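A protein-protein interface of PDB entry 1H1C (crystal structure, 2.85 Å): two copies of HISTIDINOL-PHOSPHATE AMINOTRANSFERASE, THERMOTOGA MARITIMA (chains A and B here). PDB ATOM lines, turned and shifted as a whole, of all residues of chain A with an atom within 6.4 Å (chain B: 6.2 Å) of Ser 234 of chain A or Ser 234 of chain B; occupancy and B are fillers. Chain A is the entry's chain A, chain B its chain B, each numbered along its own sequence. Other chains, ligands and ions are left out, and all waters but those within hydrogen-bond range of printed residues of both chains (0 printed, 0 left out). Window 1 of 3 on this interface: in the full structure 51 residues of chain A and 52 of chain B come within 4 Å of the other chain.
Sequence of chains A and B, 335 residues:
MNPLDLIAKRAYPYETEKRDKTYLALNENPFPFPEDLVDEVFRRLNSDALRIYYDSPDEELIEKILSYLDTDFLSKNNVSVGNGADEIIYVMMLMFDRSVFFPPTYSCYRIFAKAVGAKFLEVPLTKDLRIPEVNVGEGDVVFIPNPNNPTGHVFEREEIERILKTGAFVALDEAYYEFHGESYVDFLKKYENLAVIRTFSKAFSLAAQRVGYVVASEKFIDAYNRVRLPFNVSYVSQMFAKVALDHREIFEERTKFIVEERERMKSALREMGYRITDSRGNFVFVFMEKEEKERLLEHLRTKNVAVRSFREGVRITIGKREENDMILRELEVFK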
ATOM      1  N   TYR A  54     -39.056  12.545  23.025  1.00  0.00           N
ATOM      2  CA  TYR A  54     -38.745  11.525  24.014  1.00  0.00           C
ATOM      3  C   TYR A  54     -38.733  12.115  25.414  1.00  0.00           C
ATOM      4  O   TYR A  54     -38.348  13.265  25.611  1.00  0.00           O
ATOM      5  CB  TYR A  54     -37.375  10.918  23.688  1.00  0.00           C
ATOM      6  CG  TYR A  54     -37.031   9.642  24.416  1.00  0.00           C
ATOM      7  CD1 TYR A  54     -37.627   8.434  24.064  1.00  0.00           C
ATOM      8  CD2 TYR A  54     -36.109   9.646  25.468  1.00  0.00           C
ATOM      9  CE1 TYR A  54     -37.317   7.259  24.744  1.00  0.00           C
ATOM     10  CE2 TYR A  54     -35.793   8.482  26.155  1.00  0.00           C
ATOM     11  CZ  TYR A  54     -36.401   7.292  25.792  1.00  0.00           C
ATOM     12  OH  TYR A  54     -36.111   6.142  26.491  1.00  0.00           O
ATOM     13  N   SER A  56     -37.510  13.302  28.687  1.00  0.00           N
ATOM     14  CA  SER A  56     -36.145  13.640  29.027  1.00  0.00           C
ATOM     15  C   SER A  56     -35.819  12.716  30.191  1.00  0.00           C
ATOM     16  O   SER A  56     -35.064  11.754  30.030  1.00  0.00           O
ATOM     17  CB  SER A  56     -35.996  15.117  29.396  1.00  0.00           C
ATOM     18  OG  SER A  56     -34.643  15.521  29.234  1.00  0.00           O
ATOM     19  N   ASN A  83     -29.294  18.982  30.831  1.00  0.00           N
ATOM     20  CA  ASN A  83     -28.411  19.080  29.658  1.00  0.00           C
ATOM     21  C   ASN A  83     -27.011  19.418  30.150  1.00  0.00           C
ATOM     22  O   ASN A  83     -26.484  20.514  29.906  1.00  0.00           O
ATOM     23  CB  ASN A  83     -28.903  20.175  28.705  1.00  0.00           C
ATOM     24  CG  ASN A  83     -28.032  20.315  27.471  1.00  0.00           C
ATOM     25  OD1 ASN A  83     -27.919  19.405  26.662  1.00  0.00           O
ATOM     26  ND2 ASN A  83     -27.407  21.461  27.331  1.00  0.00           N
ATOM     27  N   ALA A 208     -19.038  15.266  25.831  1.00  0.00           N
ATOM     28  CA  ALA A 208     -19.534  15.713  24.536  1.00  0.00           C
ATOM     29  C   ALA A 208     -21.029  15.469  24.374  1.00  0.00           C
ATOM     30  O   ALA A 208     -21.660  15.989  23.439  1.00  0.00           O
ATOM     31  CB  ALA A 208     -18.786  14.969  23.431  1.00  0.00           C
ATOM     32  N   GLN A 209     -21.592  14.664  25.271  1.00  0.00           N
ATOM     33  CA  GLN A 209     -22.997  14.328  25.177  1.00  0.00           C
ATOM     34  C   GLN A 209     -23.871  14.968  26.231  1.00  0.00           C
ATOM     35  O   GLN A 209     -25.055  14.662  26.351  1.00  0.00           O
ATOM     36  CB  GLN A 209     -23.142  12.820  25.168  1.00  0.00           C
ATOM     37  CG  GLN A 209     -22.617  12.226  23.867  1.00  0.00           C
ATOM     38  CD  GLN A 209     -23.278  12.844  22.650  1.00  0.00           C
ATOM     39  OE1 GLN A 209     -24.489  12.800  22.511  1.00  0.00           O
ATOM     40  NE2 GLN A 209     -22.484  13.427  21.770  1.00  0.00           N
ATOM     41  N   ARG A 210     -23.266  15.893  26.963  1.00  0.00           N
ATOM     42  CA  ARG A 210     -23.936  16.653  27.998  1.00  0.00           C
ATOM     43  C   ARG A 210     -25.044  15.874  28.670  1.00  0.00           C
ATOM     44  O   ARG A 210     -26.171  15.856  28.188  1.00  0.00           O
ATOM     45  CB  ARG A 210     -24.503  17.926  27.384  1.00  0.00           C
ATOM     46  CG  ARG A 210     -23.699  18.444  26.187  1.00  0.00           C
ATOM     47  CD  ARG A 210     -22.300  18.908  26.550  1.00  0.00           C
ATOM     48  NE  ARG A 210     -22.342  19.901  27.608  1.00  0.00           N
ATOM     49  CZ  ARG A 210     -22.263  19.592  28.892  1.00  0.00           C
ATOM     50  NH1 ARG A 210     -22.122  18.326  29.247  1.00  0.00           N
ATOM     51  NH2 ARG A 210     -22.358  20.535  29.815  1.00  0.00           N
ATOM     52  N   VAL A 211     -24.722  15.221  29.779  1.00  0.00           N
ATOM     53  CA  VAL A 211     -25.713  14.459  30.516  1.00  0.00           C
ATOM     54  C   VAL A 211     -25.432  14.501  32.019  1.00  0.00           C
ATOM     55  O   VAL A 211     -24.514  13.840  32.515  1.00  0.00           O
ATOM     56  CB  VAL A 211     -25.756  13.006  30.031  1.00  0.00           C
ATOM     57  CG1 VAL A 211     -26.685  12.178  30.919  1.00  0.00           C
ATOM     58  CG2 VAL A 211     -26.233  12.967  28.592  1.00  0.00           C
ATOM     59  N   PHE A 231     -37.813  18.910  27.373  1.00  0.00           N
ATOM     60  CA  PHE A 231     -36.954  17.950  26.681  1.00  0.00           C
ATOM     61  C   PHE A 231     -35.501  18.450  26.639  1.00  0.00           C
ATOM     62  O   PHE A 231     -35.033  18.923  25.606  1.00  0.00           O
ATOM     63  CB  PHE A 231     -37.516  17.735  25.268  1.00  0.00           C
ATOM     64  CG  PHE A 231     -38.996  17.426  25.258  1.00  0.00           C
ATOM     65  CD1 PHE A 231     -39.936  18.444  25.206  1.00  0.00           C
ATOM     66  CD2 PHE A 231     -39.455  16.115  25.401  1.00  0.00           C
ATOM     67  CE1 PHE A 231     -41.317  18.161  25.306  1.00  0.00           C
ATOM     68  CE2 PHE A 231     -40.824  15.820  25.501  1.00  0.00           C
ATOM     69  CZ  PHE A 231     -41.755  16.843  25.455  1.00  0.00           C
ATOM     70  N   ASN A 232     -34.783  18.347  27.755  1.00  0.00           N
ATOM     71  CA  ASN A 232     -33.406  18.835  27.791  1.00  0.00           C
ATOM     72  C   ASN A 232     -32.339  17.807  27.524  1.00  0.00           C
ATOM     73  O   ASN A 232     -31.165  18.153  27.456  1.00  0.00           O
ATOM     74  CB  ASN A 232     -33.077  19.525  29.129  1.00  0.00           C
ATOM     75  CG  ASN A 232     -33.388  18.657  30.348  1.00  0.00           C
ATOM     76  OD1 ASN A 232     -32.967  18.965  31.473  1.00  0.00           O
ATOM     77  ND2 ASN A 232     -34.130  17.583  30.131  1.00  0.00           N
ATOM     78  N   VAL A 233     -32.722  16.543  27.401  1.00  0.00           N
ATOM     79  CA  VAL A 233     -31.744  15.503  27.119  1.00  0.00           C
ATOM     80  C   VAL A 233     -32.207  14.663  25.935  1.00  0.00           C
ATOM     81  O   VAL A 233     -33.301  14.096  25.950  1.00  0.00           O
ATOM     82  CB  VAL A 233     -31.516  14.613  28.348  1.00  0.00           C
ATOM     83  CG1 VAL A 233     -30.378  13.649  28.083  1.00  0.00           C
ATOM     84  CG2 VAL A 233     -31.207  15.476  29.566  1.00  0.00           C
ATOM     85  N   SER A 234     -31.370  14.605  24.902  1.00  0.00           N
ATOM     86  CA  SER A 234     -31.671  13.863  23.674  1.00  0.00           C
ATOM     87  C   SER A 234     -31.768  12.363  23.889  1.00  0.00           C
ATOM     88  O   SER A 234     -31.049  11.792  24.723  1.00  0.00           O
ATOM     89  CB  SER A 234     -30.592  14.131  22.635  1.00  0.00           C
ATOM     90  OG  SER A 234     -29.315  13.803  23.165  1.00  0.00           O
ATOM     91  N   TYR A 235     -32.652  11.723  23.120  1.00  0.00           N
ATOM     92  CA  TYR A 235     -32.850  10.275  23.206  1.00  0.00           C
ATOM     93  C   TYR A 235     -31.508   9.544  23.099  1.00  0.00           C
ATOM     94  O   TYR A 235     -31.190   8.670  23.903  1.00  0.00           O
ATOM     95  CB  TYR A 235     -33.791   9.815  22.095  1.00  0.00           C
ATOM     96  CG  TYR A 235     -33.837   8.320  21.906  1.00  0.00           C
ATOM     97  CD1 TYR A 235     -34.501   7.496  22.814  1.00  0.00           C
ATOM     98  CD2 TYR A 235     -33.208   7.724  20.811  1.00  0.00           C
ATOM     99  CE1 TYR A 235     -34.534   6.125  22.636  1.00  0.00           C
ATOM    100  CE2 TYR A 235     -33.242   6.348  20.629  1.00  0.00           C
ATOM    101  CZ  TYR A 235     -33.901   5.561  21.541  1.00  0.00           C
ATOM    102  OH  TYR A 235     -33.912   4.208  21.362  1.00  0.00           O
ATOM    103  N   VAL A 236     -30.710   9.905  22.111  1.00  0.00           N
ATOM    104  CA  VAL A 236     -29.424   9.266  21.972  1.00  0.00           C
ATOM    105  C   VAL A 236     -28.542   9.570  23.182  1.00  0.00           C
ATOM    106  O   VAL A 236     -27.831   8.692  23.644  1.00  0.00           O
ATOM    107  CB  VAL A 236     -28.709   9.726  20.672  1.00  0.00           C
ATOM    108  CG1 VAL A 236     -27.359   8.997  20.505  1.00  0.00           C
ATOM    109  CG2 VAL A 236     -29.617   9.477  19.476  1.00  0.00           C
ATOM    110  N   SER A 237     -28.580  10.795  23.701  1.00  0.00           N
ATOM    111  CA  SER A 237     -27.736  11.144  24.853  1.00  0.00           C
ATOM    112  C   SER A 237     -28.055  10.325  26.081  1.00  0.00           C
ATOM    113  O   SER A 237     -27.168   9.968  26.833  1.00  0.00           O
ATOM    114  CB  SER A 237     -27.862  12.623  25.229  1.00  0.00           C
ATOM    115  OG  SER A 237     -26.983  13.432  24.480  1.00  0.00           O
ATOM    116  N   GLN A 238     -29.328  10.040  26.302  1.00  0.00           N
ATOM    117  CA  GLN A 238     -29.672   9.251  27.464  1.00  0.00           C
ATOM    118  C   GLN A 238     -29.124   7.870  27.212  1.00  0.00           C
ATOM    119  O   GLN A 238     -28.428   7.320  28.068  1.00  0.00           O
ATOM    120  CB  GLN A 238     -31.179   9.219  27.681  1.00  0.00           C
ATOM    121  CG  GLN A 238     -31.750  10.599  27.980  1.00  0.00           C
ATOM    122  CD  GLN A 238     -33.233  10.561  28.236  1.00  0.00           C
ATOM    123  OE1 GLN A 238     -34.004  11.366  27.692  1.00  0.00           O
ATOM    124  NE2 GLN A 238     -33.648   9.621  29.070  1.00  0.00           N
ATOM    125  N   MET A 239     -29.415   7.326  26.027  1.00  0.00           N
ATOM    126  CA  MET A 239     -28.918   6.003  25.634  1.00  0.00           C
ATOM    127  C   MET A 239     -27.457   5.825  26.060  1.00  0.00           C
ATOM    128  O   MET A 239     -27.112   4.861  26.748  1.00  0.00           O
ATOM    129  CB  MET A 239     -29.028   5.821  24.126  1.00  0.00           C
ATOM    130  CG  MET A 239     -28.911   4.369  23.683  1.00  0.00           C
ATOM    131  SD  MET A 239     -30.174   3.174  24.610  1.00  0.00           S
ATOM    132  CE  MET A 239     -31.829   3.802  23.819  1.00  0.00           C
ATOM    133  N   TYR B  54     -16.991  19.277  23.154  1.00  0.00           N
ATOM    134  CA  TYR B  54     -17.104  19.639  21.752  1.00  0.00           C
ATOM    135  C   TYR B  54     -17.767  21.012  21.578  1.00  0.00           C
ATOM    136  O   TYR B  54     -18.710  21.340  22.296  1.00  0.00           O
ATOM    137  CB  TYR B  54     -17.934  18.567  21.060  1.00  0.00           C
ATOM    138  CG  TYR B  54     -17.785  18.528  19.579  1.00  0.00           C
ATOM    139  CD1 TYR B  54     -16.605  18.096  18.997  1.00  0.00           C
ATOM    140  CD2 TYR B  54     -18.834  18.897  18.752  1.00  0.00           C
ATOM    141  CE1 TYR B  54     -16.477  18.028  17.618  1.00  0.00           C
ATOM    142  CE2 TYR B  54     -18.718  18.830  17.375  1.00  0.00           C
ATOM    143  CZ  TYR B  54     -17.539  18.395  16.807  1.00  0.00           C
ATOM    144  OH  TYR B  54     -17.430  18.316  15.431  1.00  0.00           O
ATOM    145  N   SER B  56     -20.094  23.961  20.703  1.00  0.00           N
ATOM    146  CA  SER B  56     -21.547  23.945  20.523  1.00  0.00           C
ATOM    147  C   SER B  56     -21.892  24.148  19.059  1.00  0.00           C
ATOM    148  O   SER B  56     -22.223  23.181  18.375  1.00  0.00           O
ATOM    149  CB  SER B  56     -22.235  24.998  21.385  1.00  0.00           C
ATOM    150  OG  SER B  56     -23.636  24.842  21.270  1.00  0.00           O
ATOM    151  N   ASN B  83     -30.467  23.994  22.008  1.00  0.00           N
ATOM    152  CA  ASN B  83     -30.868  22.632  22.342  1.00  0.00           C
ATOM    153  C   ASN B  83     -32.359  22.566  22.030  1.00  0.00           C
ATOM    154  O   ASN B  83     -33.205  22.633  22.917  1.00  0.00           O
ATOM    155  CB  ASN B  83     -30.619  22.376  23.826  1.00  0.00           C
ATOM    156  CG  ASN B  83     -30.906  20.945  24.235  1.00  0.00           C
ATOM    157  OD1 ASN B  83     -31.126  20.662  25.417  1.00  0.00           O
ATOM    158  ND2 ASN B  83     -30.896  20.034  23.266  1.00  0.00           N
ATOM    159  N   ALA B 208     -36.272  14.081  18.930  1.00  0.00           N
ATOM    160  CA  ALA B 208     -35.680  13.498  20.133  1.00  0.00           C
ATOM    161  C   ALA B 208     -34.217  13.912  20.319  1.00  0.00           C
ATOM    162  O   ALA B 208     -33.625  13.692  21.388  1.00  0.00           O
ATOM    163  CB  ALA B 208     -35.785  11.989  20.083  1.00  0.00           C
ATOM    164  N   GLN B 209     -33.643  14.521  19.283  1.00  0.00           N
ATOM    165  CA  GLN B 209     -32.246  14.933  19.338  1.00  0.00           C
ATOM    166  C   GLN B 209     -32.026  16.383  19.743  1.00  0.00           C
ATOM    167  O   GLN B 209     -30.904  16.824  20.007  1.00  0.00           O
ATOM    168  CB  GLN B 209     -31.571  14.597  18.014  1.00  0.00           C
ATOM    169  CG  GLN B 209     -31.400  13.089  17.857  1.00  0.00           C
ATOM    170  CD  GLN B 209     -30.876  12.434  19.139  1.00  0.00           C
ATOM    171  OE1 GLN B 209     -29.737  12.666  19.542  1.00  0.00           O
ATOM    172  NE2 GLN B 209     -31.714  11.629  19.787  1.00  0.00           N
ATOM    173  N   ARG B 210     -33.130  17.109  19.809  1.00  0.00           N
ATOM    174  CA  ARG B 210     -33.136  18.493  20.238  1.00  0.00           C
ATOM    175  C   ARG B 210     -32.112  19.400  19.558  1.00  0.00           C
ATOM    176  O   ARG B 210     -31.120  19.810  20.162  1.00  0.00           O
ATOM    177  CB  ARG B 210     -32.960  18.532  21.761  1.00  0.00           C
ATOM    178  CG  ARG B 210     -33.657  17.378  22.536  1.00  0.00           C
ATOM    179  CD  ARG B 210     -35.191  17.371  22.422  1.00  0.00           C
ATOM    180  NE  ARG B 210     -35.768  18.692  22.634  1.00  0.00           N
ATOM    181  CZ  ARG B 210     -36.375  19.386  21.682  1.00  0.00           C
ATOM    182  NH1 ARG B 210     -36.861  20.582  21.944  1.00  0.00           N
ATOM    183  NH2 ARG B 210     -36.510  18.871  20.469  1.00  0.00           N
ATOM    184  N   PHE B 231     -21.942  24.787  25.872  1.00  0.00           N
ATOM    185  CA  PHE B 231     -22.119  23.555  25.111  1.00  0.00           C
ATOM    186  C   PHE B 231     -23.519  23.030  25.233  1.00  0.00           C
ATOM    187  O   PHE B 231     -23.764  22.066  25.965  1.00  0.00           O
ATOM    188  CB  PHE B 231     -21.142  22.518  25.637  1.00  0.00           C
ATOM    189  CG  PHE B 231     -19.787  23.072  25.842  1.00  0.00           C
ATOM    190  CD1 PHE B 231     -19.312  23.321  27.114  1.00  0.00           C
ATOM    191  CD2 PHE B 231     -19.036  23.499  24.749  1.00  0.00           C
ATOM    192  CE1 PHE B 231     -18.101  24.005  27.293  1.00  0.00           C
ATOM    193  CE2 PHE B 231     -17.833  24.178  24.927  1.00  0.00           C
ATOM    194  CZ  PHE B 231     -17.369  24.433  26.202  1.00  0.00           C
ATOM    195  N   ASN B 232     -24.436  23.637  24.493  1.00  0.00           N
ATOM    196  CA  ASN B 232     -25.834  23.237  24.572  1.00  0.00           C
ATOM    197  C   ASN B 232     -26.332  22.233  23.543  1.00  0.00           C
ATOM    198  O   ASN B 232     -27.508  21.911  23.541  1.00  0.00           O
ATOM    199  CB  ASN B 232     -26.723  24.488  24.524  1.00  0.00           C
ATOM    200  CG  ASN B 232     -26.625  25.243  23.194  1.00  0.00           C
ATOM    201  OD1 ASN B 232     -27.273  26.266  23.012  1.00  0.00           O
ATOM    202  ND2 ASN B 232     -25.829  24.732  22.266  1.00  0.00           N
ATOM    203  N   VAL B 233     -25.455  21.725  22.687  1.00  0.00           N
ATOM    204  CA  VAL B 233     -25.878  20.785  21.656  1.00  0.00           C
ATOM    205  C   VAL B 233     -24.872  19.648  21.494  1.00  0.00           C
ATOM    206  O   VAL B 233     -23.836  19.810  20.855  1.00  0.00           O
ATOM    207  CB  VAL B 233     -26.011  21.525  20.338  1.00  0.00           C
ATOM    208  CG1 VAL B 233     -27.366  22.227  20.247  1.00  0.00           C
ATOM    209  CG2 VAL B 233     -24.871  22.573  20.267  1.00  0.00           C
ATOM    210  N   SER B 234     -25.181  18.500  22.080  1.00  0.00           N
ATOM    211  CA  SER B 234     -24.314  17.323  22.029  1.00  0.00           C
ATOM    212  C   SER B 234     -23.594  17.087  20.707  1.00  0.00           C
ATOM    213  O   SER B 234     -24.065  17.479  19.636  1.00  0.00           O
ATOM    214  CB  SER B 234     -25.115  16.066  22.380  1.00  0.00           C
ATOM    215  OG  SER B 234     -26.341  16.016  21.667  1.00  0.00           O
ATOM    216  N   TYR B 235     -22.433  16.451  20.807  1.00  0.00           N
ATOM    217  CA  TYR B 235     -21.634  16.134  19.635  1.00  0.00           C
ATOM    218  C   TYR B 235     -22.555  15.369  18.712  1.00  0.00           C
ATOM    219  O   TYR B 235     -22.950  15.865  17.653  1.00  0.00           O
ATOM    220  CB  TYR B 235     -20.455  15.251  20.041  1.00  0.00           C
ATOM    221  CG  TYR B 235     -19.643  14.674  18.906  1.00  0.00           C
ATOM    222  CD1 TYR B 235     -18.958  15.499  18.027  1.00  0.00           C
ATOM    223  CD2 TYR B 235     -19.505  13.288  18.755  1.00  0.00           C
ATOM    224  CE1 TYR B 235     -18.152  14.964  17.028  1.00  0.00           C
ATOM    225  CE2 TYR B 235     -18.697  12.739  17.762  1.00  0.00           C
ATOM    226  CZ  TYR B 235     -18.023  13.582  16.900  1.00  0.00           C
ATOM    227  OH  TYR B 235     -17.226  13.061  15.897  1.00  0.00           O
ATOM    228  N   VAL B 236     -22.921  14.166  19.142  1.00  0.00           N
ATOM    229  CA  VAL B 236     -23.791  13.308  18.363  1.00  0.00           C
ATOM    230  C   VAL B 236     -25.007  14.013  17.761  1.00  0.00           C
ATOM    231  O   VAL B 236     -25.441  13.665  16.662  1.00  0.00           O
ATOM    232  CB  VAL B 236     -24.250  12.122  19.214  1.00  0.00           C
ATOM    233  CG1 VAL B 236     -25.254  11.267  18.449  1.00  0.00           C
ATOM    234  CG2 VAL B 236     -23.053  11.304  19.583  1.00  0.00           C
ATOM    235  N   SER B 237     -25.555  15.009  18.455  1.00  0.00           N
ATOM    236  CA  SER B 237     -26.729  15.690  17.919  1.00  0.00           C
ATOM    237  C   SER B 237     -26.467  16.542  16.697  1.00  0.00           C
ATOM    238  O   SER B 237     -27.256  16.523  15.763  1.00  0.00           O
ATOM    239  CB  SER B 237     -27.412  16.518  18.999  1.00  0.00           C
ATOM    240  OG  SER B 237     -28.096  15.661  19.906  1.00  0.00           O
ATOM    241  N   GLN B 238     -25.365  17.284  16.681  1.00  0.00           N
ATOM    242  CA  GLN B 238     -25.056  18.113  15.520  1.00  0.00           C
ATOM    243  C   GLN B 238     -24.790  17.189  14.322  1.00  0.00           C
ATOM    244  O   GLN B 238     -25.163  17.493  13.187  1.00  0.00           O
ATOM    245  CB  GLN B 238     -23.842  19.000  15.816  1.00  0.00           C
ATOM    246  CG  GLN B 238     -23.801  19.536  17.264  1.00  0.00           C
ATOM    247  CD  GLN B 238     -22.679  20.544  17.499  1.00  0.00           C
ATOM    248  OE1 GLN B 238     -22.133  20.648  18.596  1.00  0.00           O
ATOM    249  NE2 GLN B 238     -22.343  21.301  16.469  1.00  0.00           N
ATOM    250  N   MET B 239     -24.159  16.048  14.579  1.00  0.00           N
ATOM    251  CA  MET B 239     -23.877  15.082  13.520  1.00  0.00           C
ATOM    252  C   MET B 239     -25.162  14.765  12.764  1.00  0.00           C
ATOM    253  O   MET B 239     -25.194  14.792  11.534  1.00  0.00           O
ATOM    254  CB  MET B 239     -23.310  13.793  14.115  1.00  0.00           C
ATOM    255  CG  MET B 239     -22.532  12.969  13.097  1.00  0.00           C
ATOM    256  SD  MET B 239     -21.051  13.976  12.334  1.00  0.00           S
ATOM    257  CE  MET B 239     -19.701  13.414  13.645  1.00  0.00           C
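The backbone carbonyl oxygen (O) of Ala 208 of chain A sits at hydrogen-bond distance from the backbone NH (N) of Tyr 235 of chain B, at 2.8 Å.
N of Tyr 235 of chain B lies close to NE2 of Gln 209 of chain A, 3.2 Å away.
The side-chain amide nitrogen of Gln 209 of chain A lies close to the backbone NH of Val 236 of chain B (2.8 Å).
NE of Arg 210 of chain A lies within hydrogen-bond range of O of Phe 231 of chain B (3.1 Å).
The backbone carbonyl oxygen of Phe 231 of chain A is in hydrogen-bond range of the guanidinium group of Arg 210 of chain B, at 3.1 Å.
The side-chain amide oxygen of Asn 83 of chain B sits close to the backbone carbonyl oxygen of Asn 232 of chain A (3.2 Å).
The backbone NH (N) of Tyr 235 of chain A sits at hydrogen-bond distance from the backbone carbonyl oxygen (O) of Ala 208 of chain B (2.8 Å).
N of Tyr 235 of chain A lies close to NE2 of Gln 209 of chain B (3.5 Å).
The backbone NH of Val 236 of chain A lies close to the side-chain amide nitrogen of Gln 209 of chain B (3.1 Å).
The side-chain hydroxyl (OG) of Ser 56 of chain A sits at hydrogen-bond distance from the backbone NH (N) of Asn 232 of chain A, at 3.2 Å.
O of Gln 209 of chain A sits at hydrogen-bond distance from OG of Ser 237 of chain A (3.0 Å).
The side-chain hydroxyl (OG) of Ser 237 of chain A is in hydrogen-bond range of the side-chain hydroxyl (OG) of Ser 234 of chain A (2.7 Å).
OG of Ser 56 of chain B lies within hydrogen-bond range of ND2 of Asn 232 of chain B, at 2.4 Å.
The side-chain amide nitrogen (ND2) of Asn 83 of chain B lies close to the backbone carbonyl oxygen (O) of Arg 210 of chain B (3.1 Å).
The backbone carbonyl oxygen (O) of Gln 209 of chain B sits at hydrogen-bond distance from the side-chain hydroxyl (OG) of Ser 237 of chain B (3.0 Å).
Among the printed residues, pairs that only touch across the chains: Ser 234 of chain A with Ala 208 of chain B, Ala 208 of chain A with Ser 234 of chain B, Gln 209 of chain A with Ser 234 of chain B, Ser 234 of chain A with Gln 209 of chain B, Asn 83 of chain A with Asn 232 of chain B, Asn 83 of chain A with Asn 83 of chain B, Val 236 of chain A with Val 236 of chain B, Ser 237 of chain A with Ser 234 of chain B, Asn 83 of chain A with Phe 231 of chain B, Ser 234 of chain A with Ser 237 of chain B and Ser 234 of chain A with Ser 234 of chain B.
Of the printed residues of chain B, Ser 234 of chain A touches Ala 208, Gln 209, Ser 234 and Ser 237.
Of the printed residues of chain A, Ser 234 of chain B touches Ala 208 (3.3 Å), Gln 209 (3.3 Å), Ser 234 (3.998 Å) and Ser 237 (3.9 Å).
Printed residues of chain A within 4 Å of Ala 208 of chain B: Ser 234 (3.0 Å) and Tyr 235 (2.8 Å).
Printed residues of chain B within 4 Å of Asn 232 of chain A: Asn 83.
The nearest printed residue of chain B that does not touch Ser 234 of chain A is Arg 210 of chain B (4.2 Å).
Along chain A the printed residues that touch a printed residue of chain B span positions 83 to 237.
Hydrophobic or aromatic side chains of chain B within 4 Å of the printed part of chain A: Ala 208, Phe 231, Tyr 235 and Val 236.
Among the printed residues, no Asp or Glu carboxylate lies within 4 Å of a Lys or Arg side-chain nitrogen of the other chain.
Asn 83 of chain A touches its own counterpart, Asn 83 of chain B.
Gln 209 of chain A touches Val 236 of chain B, and with the chains exchanged Val 236 of chain A touches Gln 209 of chain B.
Ser 234 of chain B touches its own counterpart, Ser 234 of chain A.
Val 236 of chain A touches its own counterpart, Val 236 of chain B.
Of the 20 pairs that touch across the chains among the printed residues, 19 have their exchanged pair printed and touching as well.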
